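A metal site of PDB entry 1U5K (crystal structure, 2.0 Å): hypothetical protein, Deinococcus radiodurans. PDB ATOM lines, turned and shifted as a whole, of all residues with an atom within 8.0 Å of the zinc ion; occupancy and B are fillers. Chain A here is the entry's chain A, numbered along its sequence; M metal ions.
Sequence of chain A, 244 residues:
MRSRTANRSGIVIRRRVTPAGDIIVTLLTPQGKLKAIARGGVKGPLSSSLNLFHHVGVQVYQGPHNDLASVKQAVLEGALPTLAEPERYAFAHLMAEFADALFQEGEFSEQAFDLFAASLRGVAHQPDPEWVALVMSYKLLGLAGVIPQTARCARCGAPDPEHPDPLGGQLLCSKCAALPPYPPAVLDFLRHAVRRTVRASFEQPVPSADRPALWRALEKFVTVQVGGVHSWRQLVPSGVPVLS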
ATOM      1  N   ARG A 152      -7.961  14.791   5.402  1.00  0.00           N
ATOM      2  CA  ARG A 152      -7.729  16.199   5.701  1.00  0.00           C
ATOM      3  C   ARG A 152      -7.356  17.035   4.482  1.00  0.00           C
ATOM      4  O   ARG A 152      -6.727  16.551   3.554  1.00  0.00           O
ATOM      5  CB  ARG A 152      -6.624  16.315   6.752  1.00  0.00           C
ATOM      6  CG  ARG A 152      -6.943  15.655   8.089  1.00  0.00           C
ATOM      7  CD  ARG A 152      -5.820  15.880   9.086  1.00  0.00           C
ATOM      8  NE  ARG A 152      -6.140  15.586  10.480  1.00  0.00           N
ATOM      9  CZ  ARG A 152      -6.879  16.312  11.321  1.00  0.00           C
ATOM     10  NH1 ARG A 152      -7.489  17.435  10.966  1.00  0.00           N
ATOM     11  NH2 ARG A 152      -7.037  15.856  12.557  1.00  0.00           N
ATOM     12  N   CYS A 153      -7.765  18.303   4.475  1.00  0.00           N
ATOM     13  CA  CYS A 153      -7.422  19.208   3.398  1.00  0.00           C
ATOM     14  C   CYS A 153      -5.910  19.226   3.243  1.00  0.00           C
ATOM     15  O   CYS A 153      -5.169  19.353   4.217  1.00  0.00           O
ATOM     16  CB  CYS A 153      -7.944  20.619   3.680  1.00  0.00           C
ATOM     17  SG  CYS A 153      -7.335  21.922   2.602  1.00  0.00           S
ATOM     18  N   ALA A 154      -5.456  19.107   2.004  1.00  0.00           N
ATOM     19  CA  ALA A 154      -4.031  19.013   1.707  1.00  0.00           C
ATOM     20  C   ALA A 154      -3.318  20.334   2.022  1.00  0.00           C
ATOM     21  O   ALA A 154      -2.102  20.346   2.152  1.00  0.00           O
ATOM     22  CB  ALA A 154      -3.829  18.655   0.248  1.00  0.00           C
ATOM     23  N   ARG A 155      -4.053  21.433   2.159  1.00  0.00           N
ATOM     24  CA  ARG A 155      -3.407  22.713   2.440  1.00  0.00           C
ATOM     25  C   ARG A 155      -3.456  23.074   3.927  1.00  0.00           C
ATOM     26  O   ARG A 155      -2.411  23.253   4.545  1.00  0.00           O
ATOM     27  CB  ARG A 155      -4.033  23.802   1.571  1.00  0.00           C
ATOM     28  CG  ARG A 155      -3.525  25.207   1.798  1.00  0.00           C
ATOM     29  CD  ARG A 155      -3.858  26.163   0.681  1.00  0.00           C
ATOM     30  NE  ARG A 155      -3.354  27.539   0.807  1.00  0.00           N
ATOM     31  CZ  ARG A 155      -4.042  28.542   1.354  1.00  0.00           C
ATOM     32  NH1 ARG A 155      -5.205  28.322   1.930  1.00  0.00           N
ATOM     33  NH2 ARG A 155      -3.572  29.784   1.338  1.00  0.00           N
ATOM     34  N   CYS A 156      -4.646  23.218   4.508  1.00  0.00           N
ATOM     35  CA  CYS A 156      -4.778  23.658   5.884  1.00  0.00           C
ATOM     36  C   CYS A 156      -5.033  22.558   6.911  1.00  0.00           C
ATOM     37  O   CYS A 156      -4.974  22.808   8.115  1.00  0.00           O
ATOM     38  CB  CYS A 156      -5.922  24.657   5.992  1.00  0.00           C
ATOM     39  SG  CYS A 156      -7.576  23.939   5.938  1.00  0.00           S
ATOM     40  N   GLY A 157      -5.402  21.365   6.463  1.00  0.00           N
ATOM     41  CA  GLY A 157      -5.580  20.235   7.343  1.00  0.00           C
ATOM     42  C   GLY A 157      -6.980  19.995   7.844  1.00  0.00           C
ATOM     43  O   GLY A 157      -7.155  19.041   8.595  1.00  0.00           O
ATOM     44  N   ALA A 158      -7.941  20.832   7.476  1.00  0.00           N
ATOM     45  CA  ALA A 158      -9.341  20.664   7.857  1.00  0.00           C
ATOM     46  C   ALA A 158      -9.929  19.303   7.490  1.00  0.00           C
ATOM     47  O   ALA A 158      -9.669  18.741   6.423  1.00  0.00           O
ATOM     48  CB  ALA A 158     -10.240  21.746   7.300  1.00  0.00           C
ATOM     49  N   PRO A 159     -10.675  18.744   8.429  1.00  0.00           N
ATOM     50  CA  PRO A 159     -11.238  17.398   8.253  1.00  0.00           C
ATOM     51  C   PRO A 159     -12.246  17.286   7.114  1.00  0.00           C
ATOM     52  O   PRO A 159     -13.015  18.215   6.845  1.00  0.00           O
ATOM     53  CB  PRO A 159     -11.816  17.044   9.627  1.00  0.00           C
ATOM     54  CG  PRO A 159     -11.636  18.227  10.478  1.00  0.00           C
ATOM     55  CD  PRO A 159     -10.926  19.334   9.755  1.00  0.00           C
ATOM     56  N   PRO A 161     -12.291  17.078   3.562  1.00  0.00           N
ATOM     57  CA  PRO A 161     -12.360  17.968   2.407  1.00  0.00           C
ATOM     58  C   PRO A 161     -13.178  17.351   1.275  1.00  0.00           C
ATOM     59  O   PRO A 161     -13.138  16.136   1.053  1.00  0.00           O
ATOM     60  CB  PRO A 161     -10.891  18.095   1.994  1.00  0.00           C
ATOM     61  CG  PRO A 161     -10.237  16.844   2.437  1.00  0.00           C
ATOM     62  CD  PRO A 161     -10.961  16.479   3.712  1.00  0.00           C
ATOM     63  N   LEU A 171      -7.204  16.305  -1.879  1.00  0.00           N
ATOM     64  CA  LEU A 171      -8.460  17.043  -1.734  1.00  0.00           C
ATOM     65  C   LEU A 171      -8.296  18.308  -0.889  1.00  0.00           C
ATOM     66  O   LEU A 171      -7.455  18.343   0.005  1.00  0.00           O
ATOM     67  CB  LEU A 171      -9.498  16.148  -1.074  1.00  0.00           C
ATOM     68  CG  LEU A 171      -9.852  14.826  -1.765  1.00  0.00           C
ATOM     69  CD1 LEU A 171     -10.631  14.008  -0.781  1.00  0.00           C
ATOM     70  CD2 LEU A 171     -10.641  15.064  -3.030  1.00  0.00           C
ATOM     71  N   LEU A 172      -9.076  19.338  -1.170  1.00  0.00           N
ATOM     72  CA  LEU A 172      -9.052  20.628  -0.483  1.00  0.00           C
ATOM     73  C   LEU A 172     -10.400  20.889   0.187  1.00  0.00           C
ATOM     74  O   LEU A 172     -11.430  20.447  -0.327  1.00  0.00           O
ATOM     75  CB  LEU A 172      -8.758  21.775  -1.442  1.00  0.00           C
ATOM     76  CG  LEU A 172      -7.375  21.733  -2.073  1.00  0.00           C
ATOM     77  CD1 LEU A 172      -7.261  22.785  -3.160  1.00  0.00           C
ATOM     78  CD2 LEU A 172      -6.299  21.823  -1.008  1.00  0.00           C
ATOM     79  N   CYS A 173     -10.387  21.647   1.286  1.00  0.00           N
ATOM     80  CA  CYS A 173     -11.632  22.091   1.904  1.00  0.00           C
ATOM     81  C   CYS A 173     -12.237  23.249   1.135  1.00  0.00           C
ATOM     82  O   CYS A 173     -11.599  23.864   0.267  1.00  0.00           O
ATOM     83  CB  CYS A 173     -11.435  22.487   3.373  1.00  0.00           C
ATOM     84  SG  CYS A 173     -10.532  24.042   3.603  1.00  0.00           S
ATOM     85  N   SER A 174     -13.480  23.584   1.487  1.00  0.00           N
ATOM     86  CA  SER A 174     -14.243  24.634   0.823  1.00  0.00           C
ATOM     87  C   SER A 174     -13.535  25.984   0.923  1.00  0.00           C
ATOM     88  O   SER A 174     -13.639  26.806   0.022  1.00  0.00           O
ATOM     89  CB  SER A 174     -15.673  24.695   1.344  1.00  0.00           C
ATOM     90  OG  SER A 174     -15.717  25.199   2.681  1.00  0.00           O
ATOM     91  N   LYS A 175     -12.742  26.201   1.973  1.00  0.00           N
ATOM     92  CA  LYS A 175     -12.040  27.461   2.132  1.00  0.00           C
ATOM     93  C   LYS A 175     -10.759  27.554   1.306  1.00  0.00           C
ATOM     94  O   LYS A 175     -10.440  28.639   0.838  1.00  0.00           O
ATOM     95  CB  LYS A 175     -11.737  27.712   3.611  1.00  0.00           C
ATOM     96  CG  LYS A 175     -12.950  27.846   4.525  1.00  0.00           C
ATOM     97  CD  LYS A 175     -13.767  29.112   4.380  1.00  0.00           C
ATOM     98  CE  LYS A 175     -14.768  29.286   5.556  1.00  0.00           C
ATOM     99  NZ  LYS A 175     -14.245  30.199   6.654  1.00  0.00           N
ATOM    100  N   CYS A 176     -10.074  26.450   1.058  1.00  0.00           N
ATOM    101  CA  CYS A 176      -8.821  26.462   0.315  1.00  0.00           C
ATOM    102  C   CYS A 176      -9.072  26.296  -1.187  1.00  0.00           C
ATOM    103  O   CYS A 176      -8.242  26.643  -2.003  1.00  0.00           O
ATOM    104  CB  CYS A 176      -7.895  25.377   0.846  1.00  0.00           C
ATOM    105  SG  CYS A 176      -7.260  25.704   2.501  1.00  0.00           S
ATOM    106  N   ALA A 177     -10.261  25.834  -1.554  1.00  0.00           N
ATOM    107  CA  ALA A 177     -10.591  25.455  -2.918  1.00  0.00           C
ATOM    108  C   ALA A 177     -11.146  26.629  -3.727  1.00  0.00           C
ATOM    109  O   ALA A 177     -11.800  27.529  -3.205  1.00  0.00           O
ATOM    110  CB  ALA A 177     -11.593  24.322  -2.896  1.00  0.00           C
HETATM  111 ZN    ZN M   1      -8.225  23.884   3.740  1.00  0.00          ZN
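N of Ala 158 lies close to SG of Cys 156.
The side-chain sulfur (SG) of Cys 173 lies close to the backbone NH (N) of Lys 175 (3.5 Å).
SG of Cys 176 lies close to NH1 of Arg 155 (3.4 Å).
The backbone carbonyl oxygen (O) of Ala 158 sits at hydrogen-bond distance from the backbone NH (N) of Cys 153 (2.8 Å).
The backbone NH (N) of Arg 155 sits close to the side-chain sulfur (SG) of Cys 153, 3.3 Å away.
Four residues have an atom within 4 Å of the zinc ion: Cys 153, Cys 156, Cys 173 and Cys 176.
The side-chain sulfur (SG) of Cys 156 is bound to the zinc ion.
The zinc ion is bound by SG of Cys 173 (2.3 Å).
SG of Cys 176 binds the zinc ion.
SG of Cys 153 is bound to the zinc ion (2.4 Å).
The zinc ion has four donor atoms within binding distance.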
